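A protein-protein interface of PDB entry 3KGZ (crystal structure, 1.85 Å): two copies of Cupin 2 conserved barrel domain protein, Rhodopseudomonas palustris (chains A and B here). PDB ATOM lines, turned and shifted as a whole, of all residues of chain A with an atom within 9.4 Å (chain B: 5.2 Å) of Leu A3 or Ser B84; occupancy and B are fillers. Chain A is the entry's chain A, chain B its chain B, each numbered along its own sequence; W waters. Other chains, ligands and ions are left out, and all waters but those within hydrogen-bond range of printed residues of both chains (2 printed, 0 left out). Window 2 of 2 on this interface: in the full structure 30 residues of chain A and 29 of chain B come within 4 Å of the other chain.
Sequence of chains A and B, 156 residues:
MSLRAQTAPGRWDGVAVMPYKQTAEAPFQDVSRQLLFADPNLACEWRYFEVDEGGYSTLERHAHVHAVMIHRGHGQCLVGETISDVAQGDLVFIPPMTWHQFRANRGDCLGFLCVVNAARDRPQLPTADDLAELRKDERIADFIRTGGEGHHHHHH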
ATOM      1  N   SER A   2      22.743  30.866  -4.122  1.00  0.00           N
ATOM      2  CA  SER A   2      21.358  30.278  -4.035  1.00  0.00           C
ATOM      3  C   SER A   2      20.847  29.965  -5.449  1.00  0.00           C
ATOM      4  O   SER A   2      21.219  30.666  -6.405  1.00  0.00           O
ATOM      5  CB  SER A   2      20.405  31.263  -3.370  1.00  0.00           C
ATOM      6  OG  SER A   2      20.140  32.420  -4.188  1.00  0.00           O
ATOM      7  N   LEU A   3      20.043  28.921  -5.571  1.00  0.00           N
ATOM      8  CA  LEU A   3      19.378  28.575  -6.819  1.00  0.00           C
ATOM      9  C   LEU A   3      17.890  28.456  -6.600  1.00  0.00           C
ATOM     10  O   LEU A   3      17.439  27.769  -5.678  1.00  0.00           O
ATOM     11  CB  LEU A   3      19.902  27.233  -7.351  1.00  0.00           C
ATOM     12  CG  LEU A   3      19.149  26.604  -8.523  1.00  0.00           C
ATOM     13  CD1 LEU A   3      19.412  27.344  -9.873  1.00  0.00           C
ATOM     14  CD2 LEU A   3      19.582  25.151  -8.606  1.00  0.00           C
ATOM     15  N   ARG A   4      17.126  29.096  -7.468  1.00  0.00           N
ATOM     16  CA  ARG A   4      15.689  28.918  -7.515  1.00  0.00           C
ATOM     17  C   ARG A   4      15.366  28.580  -8.979  1.00  0.00           C
ATOM     18  O   ARG A   4      15.382  29.424  -9.884  1.00  0.00           O
ATOM     19  CB  ARG A   4      14.996  30.179  -7.026  1.00  0.00           C
ATOM     20  CG  ARG A   4      15.098  30.403  -5.505  1.00  0.00           C
ATOM     21  CD  ARG A   4      14.732  31.829  -5.099  1.00  0.00           C
ATOM     22  NE  ARG A   4      15.727  32.745  -5.625  1.00  0.00           N
ATOM     23  CZ  ARG A   4      15.497  34.039  -5.916  1.00  0.00           C
ATOM     24  NH1 ARG A   4      14.318  34.606  -5.710  1.00  0.00           N
ATOM     25  NH2 ARG A   4      16.455  34.737  -6.463  1.00  0.00           N
ATOM     26  N   ALA A   5      15.093  27.308  -9.227  1.00  0.00           N
ATOM     27  CA  ALA A   5      14.949  26.854 -10.600  1.00  0.00           C
ATOM     28  C   ALA A   5      13.623  27.267 -11.212  1.00  0.00           C
ATOM     29  O   ALA A   5      12.622  27.311 -10.512  1.00  0.00           O
ATOM     30  CB  ALA A   5      15.115  25.306 -10.651  1.00  0.00           C
ATOM     31  N   GLN A   6      13.591  27.574 -12.509  1.00  0.00           N
ATOM     32  CA  GLN A   6      12.330  27.770 -13.207  1.00  0.00           C
ATOM     33  C   GLN A   6      11.567  26.448 -13.170  1.00  0.00           C
ATOM     34  O   GLN A   6      12.172  25.402 -13.398  1.00  0.00           O
ATOM     35  CB  GLN A   6      12.566  28.170 -14.669  1.00  0.00           C
ATOM     36  CG  GLN A   6      11.320  28.018 -15.528  1.00  0.00           C
ATOM     37  CD  GLN A   6      11.490  28.559 -16.906  1.00  0.00           C
ATOM     38  OE1 GLN A   6      11.633  29.754 -17.093  1.00  0.00           O
ATOM     39  NE2 GLN A   6      11.466  27.668 -17.903  1.00  0.00           N
ATOM     40  N   TRP A  12       8.833  29.891 -10.552  1.00  0.00           N
ATOM     41  CA  TRP A  12      10.072  29.447  -9.969  1.00  0.00           C
ATOM     42  C   TRP A  12       9.852  28.794  -8.597  1.00  0.00           C
ATOM     43  O   TRP A  12       9.001  29.207  -7.809  1.00  0.00           O
ATOM     44  CB  TRP A  12      11.070  30.595  -9.833  1.00  0.00           C
ATOM     45  CG  TRP A  12      11.465  31.303 -11.084  1.00  0.00           C
ATOM     46  CD1 TRP A  12      12.599  31.092 -11.807  1.00  0.00           C
ATOM     47  CD2 TRP A  12      10.780  32.384 -11.740  1.00  0.00           C
ATOM     48  NE1 TRP A  12      12.628  31.928 -12.883  1.00  0.00           N
ATOM     49  CE2 TRP A  12      11.515  32.708 -12.885  1.00  0.00           C
ATOM     50  CE3 TRP A  12       9.577  33.039 -11.524  1.00  0.00           C
ATOM     51  CZ2 TRP A  12      11.137  33.742 -13.755  1.00  0.00           C
ATOM     52  CZ3 TRP A  12       9.190  34.050 -12.396  1.00  0.00           C
ATOM     53  CH2 TRP A  12       9.971  34.388 -13.487  1.00  0.00           C
ATOM     54  N   ASP A  13      10.629  27.769  -8.344  1.00  0.00           N
ATOM     55  CA  ASP A  13      10.712  27.111  -7.033  1.00  0.00           C
ATOM     56  C   ASP A  13      11.154  28.147  -6.018  1.00  0.00           C
ATOM     57  O   ASP A  13      12.180  28.802  -6.179  1.00  0.00           O
ATOM     58  CB  ASP A  13      11.734  26.001  -7.091  1.00  0.00           C
ATOM     59  CG  ASP A  13      11.907  25.231  -5.780  1.00  0.00           C
ATOM     60  OD1 ASP A  13      10.946  24.988  -5.066  1.00  0.00           O
ATOM     61  OD2 ASP A  13      13.056  24.828  -5.514  1.00  0.00           O
ATOM     62  N   GLY A  14      10.362  28.266  -4.982  1.00  0.00           N
ATOM     63  CA  GLY A  14      10.660  29.177  -3.882  1.00  0.00           C
ATOM     64  C   GLY A  14      10.330  30.627  -4.169  1.00  0.00           C
ATOM     65  O   GLY A  14      10.807  31.520  -3.430  1.00  0.00           O
ATOM     66  N   VAL A  15       9.528  30.881  -5.213  1.00  0.00           N
ATOM     67  CA  VAL A  15       9.072  32.225  -5.502  1.00  0.00           C
ATOM     68  C   VAL A  15       7.561  32.209  -5.518  1.00  0.00           C
ATOM     69  O   VAL A  15       6.957  31.396  -6.251  1.00  0.00           O
ATOM     70  CB  VAL A  15       9.624  32.802  -6.848  1.00  0.00           C
ATOM     71  CG1 VAL A  15       9.028  34.239  -7.138  1.00  0.00           C
ATOM     72  CG2 VAL A  15      11.132  32.830  -6.860  1.00  0.00           C
ATOM     73  N   LEU A  36      11.970  38.579  -7.828  1.00  0.00           N
ATOM     74  CA  LEU A  36      13.071  37.695  -8.176  1.00  0.00           C
ATOM     75  C   LEU A  36      14.325  38.004  -7.381  1.00  0.00           C
ATOM     76  O   LEU A  36      14.926  37.112  -6.767  1.00  0.00           O
ATOM     77  CB  LEU A  36      13.337  37.727  -9.669  1.00  0.00           C
ATOM     78  CG  LEU A  36      12.123  37.496 -10.540  1.00  0.00           C
ATOM     79  CD1 LEU A  36      12.576  37.457 -12.016  1.00  0.00           C
ATOM     80  CD2 LEU A  36      11.351  36.237 -10.192  1.00  0.00           C
ATOM     81  N   PHE A  37      14.686  39.271  -7.306  1.00  0.00           N
ATOM     82  CA  PHE A  37      15.896  39.622  -6.556  1.00  0.00           C
ATOM     83  C   PHE A  37      15.695  40.934  -5.832  1.00  0.00           C
ATOM     84  O   PHE A  37      15.233  41.902  -6.409  1.00  0.00           O
ATOM     85  CB  PHE A  37      17.113  39.790  -7.434  1.00  0.00           C
ATOM     86  CG  PHE A  37      17.553  38.579  -8.130  1.00  0.00           C
ATOM     87  CD1 PHE A  37      18.438  37.693  -7.533  1.00  0.00           C
ATOM     88  CD2 PHE A  37      17.102  38.324  -9.416  1.00  0.00           C
ATOM     89  CE1 PHE A  37      18.904  36.520  -8.217  1.00  0.00           C
ATOM     90  CE2 PHE A  37      17.533  37.138 -10.092  1.00  0.00           C
ATOM     91  CZ  PHE A  37      18.423  36.261  -9.504  1.00  0.00           C
ATOM     92  N   GLY B  75      23.662  24.187 -18.445  1.00  0.00           N
ATOM     93  CA  GLY B  75      25.015  23.968 -17.993  1.00  0.00           C
ATOM     94  C   GLY B  75      25.070  23.737 -16.521  1.00  0.00           C
ATOM     95  O   GLY B  75      24.107  23.217 -15.922  1.00  0.00           O
ATOM     96  N   GLN B  76      26.196  24.126 -15.918  1.00  0.00           N
ATOM     97  CA  GLN B  76      26.388  24.006 -14.488  1.00  0.00           C
ATOM     98  C   GLN B  76      27.069  25.225 -13.948  1.00  0.00           C
ATOM     99  O   GLN B  76      27.736  25.955 -14.686  1.00  0.00           O
ATOM    100  CB  GLN B  76      27.261  22.769 -14.107  1.00  0.00           C
ATOM    101  CG  GLN B  76      26.639  21.429 -14.467  1.00  0.00           C
ATOM    102  CD  GLN B  76      27.294  20.313 -13.712  1.00  0.00           C
ATOM    103  OE1 GLN B  76      28.522  20.181 -13.724  1.00  0.00           O
ATOM    104  NE2 GLN B  76      26.491  19.551 -12.983  1.00  0.00           N
ATOM    105  N   CYS B  77      26.942  25.429 -12.654  1.00  0.00           N
ATOM    106  CA  CYS B  77      27.703  26.485 -12.003  1.00  0.00           C
ATOM    107  C   CYS B  77      28.240  26.081 -10.655  1.00  0.00           C
ATOM    108  O   CYS B  77      27.654  25.273  -9.940  1.00  0.00           O
ATOM    109  CB  CYS B  77      26.872  27.765 -11.878  1.00  0.00           C
ATOM    110  SG  CYS B  77      25.517  27.688 -10.709  1.00  0.00           S
ATOM    111  N   LEU B  78      29.384  26.641 -10.298  1.00  0.00           N
ATOM    112  CA  LEU B  78      29.868  26.561  -8.932  1.00  0.00           C
ATOM    113  C   LEU B  78      29.561  27.883  -8.316  1.00  0.00           C
ATOM    114  O   LEU B  78      29.903  28.897  -8.910  1.00  0.00           O
ATOM    115  CB  LEU B  78      31.379  26.351  -8.867  1.00  0.00           C
ATOM    116  CG  LEU B  78      32.068  26.658  -7.512  1.00  0.00           C
ATOM    117  CD1 LEU B  78      31.615  25.739  -6.354  1.00  0.00           C
ATOM    118  CD2 LEU B  78      33.594  26.557  -7.734  1.00  0.00           C
ATOM    119  N   THR B  82      28.841  24.867  -3.693  1.00  0.00           N
ATOM    120  CA  THR B  82      27.780  24.097  -4.335  1.00  0.00           C
ATOM    121  C   THR B  82      27.832  24.136  -5.847  1.00  0.00           C
ATOM    122  O   THR B  82      27.916  25.199  -6.445  1.00  0.00           O
ATOM    123  CB  THR B  82      26.416  24.633  -3.901  1.00  0.00           C
ATOM    124  OG1 THR B  82      26.325  24.615  -2.468  1.00  0.00           O
ATOM    125  CG2 THR B  82      25.281  23.827  -4.523  1.00  0.00           C
ATOM    126  N   ILE B  83      27.772  22.954  -6.457  1.00  0.00           N
ATOM    127  CA  ILE B  83      27.731  22.811  -7.899  1.00  0.00           C
ATOM    128  C   ILE B  83      26.291  22.483  -8.240  1.00  0.00           C
ATOM    129  O   ILE B  83      25.752  21.472  -7.737  1.00  0.00           O
ATOM    130  CB  ILE B  83      28.636  21.672  -8.389  1.00  0.00           C
ATOM    131  CG1 ILE B  83      30.086  21.962  -8.062  1.00  0.00           C
ATOM    132  CG2 ILE B  83      28.493  21.432  -9.922  1.00  0.00           C
ATOM    133  CD1 ILE B  83      30.996  20.800  -8.401  1.00  0.00           C
ATOM    134  N   SER B  84      25.672  23.328  -9.074  1.00  0.00           N
ATOM    135  CA  SER B  84      24.288  23.135  -9.503  1.00  0.00           C
ATOM    136  C   SER B  84      24.153  22.981 -11.004  1.00  0.00           C
ATOM    137  O   SER B  84      24.878  23.581 -11.799  1.00  0.00           O
ATOM    138  CB  SER B  84      23.418  24.323  -9.049  1.00  0.00           C
ATOM    139  OG  SER B  84      23.618  24.617  -7.687  1.00  0.00           O
ATOM    140  N   ASP B  85      23.200  22.177 -11.408  1.00  0.00           N
ATOM    141  CA  ASP B  85      22.736  22.192 -12.782  1.00  0.00           C
ATOM    142  C   ASP B  85      21.901  23.473 -12.967  1.00  0.00           C
ATOM    143  O   ASP B  85      21.068  23.811 -12.100  1.00  0.00           O
ATOM    144  CB  ASP B  85      21.855  20.982 -13.055  1.00  0.00           C
ATOM    145  CG  ASP B  85      22.591  19.650 -12.829  1.00  0.00           C
ATOM    146  OD1 ASP B  85      23.757  19.543 -13.230  1.00  0.00           O
ATOM    147  OD2 ASP B  85      21.984  18.724 -12.254  1.00  0.00           O
ATOM    148  N   VAL B  86      22.098  24.153 -14.087  1.00  0.00           N
ATOM    149  CA  VAL B  86      21.305  25.312 -14.405  1.00  0.00           C
ATOM    150  C   VAL B  86      20.730  25.232 -15.808  1.00  0.00           C
ATOM    151  O   VAL B  86      21.395  24.752 -16.739  1.00  0.00           O
ATOM    152  CB  VAL B  86      22.119  26.618 -14.214  1.00  0.00           C
ATOM    153  CG1 VAL B  86      22.450  26.806 -12.744  1.00  0.00           C
ATOM    154  CG2 VAL B  86      23.361  26.635 -15.108  1.00  0.00           C
ATOM    155  N   ASP B  90      16.508  29.742 -14.702  1.00  0.00           N
ATOM    156  CA  ASP B  90      16.896  29.528 -13.298  1.00  0.00           C
ATOM    157  C   ASP B  90      17.514  30.815 -12.703  1.00  0.00           C
ATOM    158  O   ASP B  90      18.226  31.515 -13.408  1.00  0.00           O
ATOM    159  CB  ASP B  90      17.882  28.389 -13.169  1.00  0.00           C
ATOM    160  CG  ASP B  90      17.253  27.028 -13.415  1.00  0.00           C
ATOM    161  OD1 ASP B  90      16.023  26.949 -13.757  1.00  0.00           O
ATOM    162  OD2 ASP B  90      18.041  26.050 -13.311  1.00  0.00           O
ATOM    163  N   LEU B  91      17.177  31.121 -11.448  1.00  0.00           N
ATOM    164  CA  LEU B  91      17.694  32.279 -10.740  1.00  0.00           C
ATOM    165  C   LEU B  91      18.858  31.851  -9.840  1.00  0.00           C
ATOM    166  O   LEU B  91      18.712  30.964  -8.992  1.00  0.00           O
ATOM    167  CB  LEU B  91      16.611  32.908  -9.866  1.00  0.00           C
ATOM    168  CG  LEU B  91      15.266  33.129 -10.529  1.00  0.00           C
ATOM    169  CD1 LEU B  91      14.151  33.516  -9.549  1.00  0.00           C
ATOM    170  CD2 LEU B  91      15.407  34.180 -11.574  1.00  0.00           C
ATOM    171  N   VAL B  92      19.996  32.507 -10.017  1.00  0.00           N
ATOM    172  CA  VAL B  92      21.163  32.279  -9.190  1.00  0.00           C
ATOM    173  C   VAL B  92      21.537  33.615  -8.566  1.00  0.00           C
ATOM    174  O   VAL B  92      21.730  34.614  -9.274  1.00  0.00           O
ATOM    175  CB  VAL B  92      22.315  31.725 -10.036  1.00  0.00           C
ATOM    176  CG1 VAL B  92      23.576  31.594  -9.234  1.00  0.00           C
ATOM    177  CG2 VAL B  92      21.956  30.338 -10.644  1.00  0.00           C
HETATM  178  O   HOH W   1      18.498  32.395  -6.471  1.00  0.00           O
HETATM  179  O   HOH W   2      14.657  24.829 -14.505  1.00  0.00           O
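The guanidinium group (NH1) of Arg A4 lies within hydrogen-bond range of the backbone carbonyl oxygen (O) of Leu A36.
The backbone carbonyl oxygen of Ala A5 is in hydrogen-bond range of the backbone NH of Asp A13, 3.0 Å away.
O of Ser B84 lies within hydrogen-bond range of N of Cys B77, 2.9 Å away.
Among the printed residues, merely in contact across the chains: Ser A2 with Val B92, Leu A3 with Leu B91, Ala A5 with Asp B90, Phe A37 with Val B92, Trp A12 with Leu B91, Ser A2 with Leu B91, Arg A4 with Asp B90, Leu A3 with Asp B90, Phe A37 with Leu B91, Leu A3 with Ser B84 and Leu A36 with Leu B91.
Of the 11 printed residues of chain A, 8 touch a printed residue of chain B.
Hydrophobic or aromatic side chains of chain A that line the printed part of chain B: Leu A3, Ala A5, Trp A12, Leu A36 and Phe A37.
Of the 12 printed residues of chain B, 4 touch a printed residue of chain A.
No position is printed for both chains.
Of the 13 pairs that touch across the chains among the printed residues, none has its exchanged pair printed and touching as well.
Printed residues of chain B within 4 Å of Ser A2: Leu B91 (3.6 Å) and Val B92 (3.2 Å).
Of the printed residues of chain B, Leu A3 touches Ser B84 (3.9 Å), Asp B90 (3.8 Å) and Leu B91 (3.3 Å).
Of the printed residues of chain B, Ala A5 touches Asp B90.
Printed residues of chain B within 4 Å of Trp A12: Leu B91 (3.6 Å).
No residue of chain A comes within 4 Å of Gln B76.
Of chain A, only Leu A3 comes within 4 Å of Ser B84.
Asp B85 touches none of the printed residues of chain A.
Printed residues of chain A within 4 Å of Val B92: Ser A2 and Phe A37.
The nearest printed residue of chain B that does not touch Leu A3 is Val B92 (4.004 Å).
The nearest residue of chain A that does not touch Ser B84 is Ser A2 (6.4 Å).
The nearest printed residue of chain A that does not touch Val B92 is Leu A3 (4.004 Å).
The backbone NH of Arg A4 sits at hydrogen-bond distance from the backbone carbonyl oxygen of Leu B91.
The side-chain carboxylate (OD1) of Asp B90 sits at hydrogen-bond distance from the backbone NH (N) of Gln A6, at 2.8 Å.
Water W2 bridges OD1 of Asp B90 (2.6 Å) and O of Gln A6 (2.8 Å).
Water W1 lies within hydrogen-bond range of the side-chain hydroxyl (OG) of Ser A2 (2.8 Å), the backbone carbonyl oxygen (O) of Leu B91 (2.9 Å) and the guanidinium group (NE) of Arg A4 (2.9 Å).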
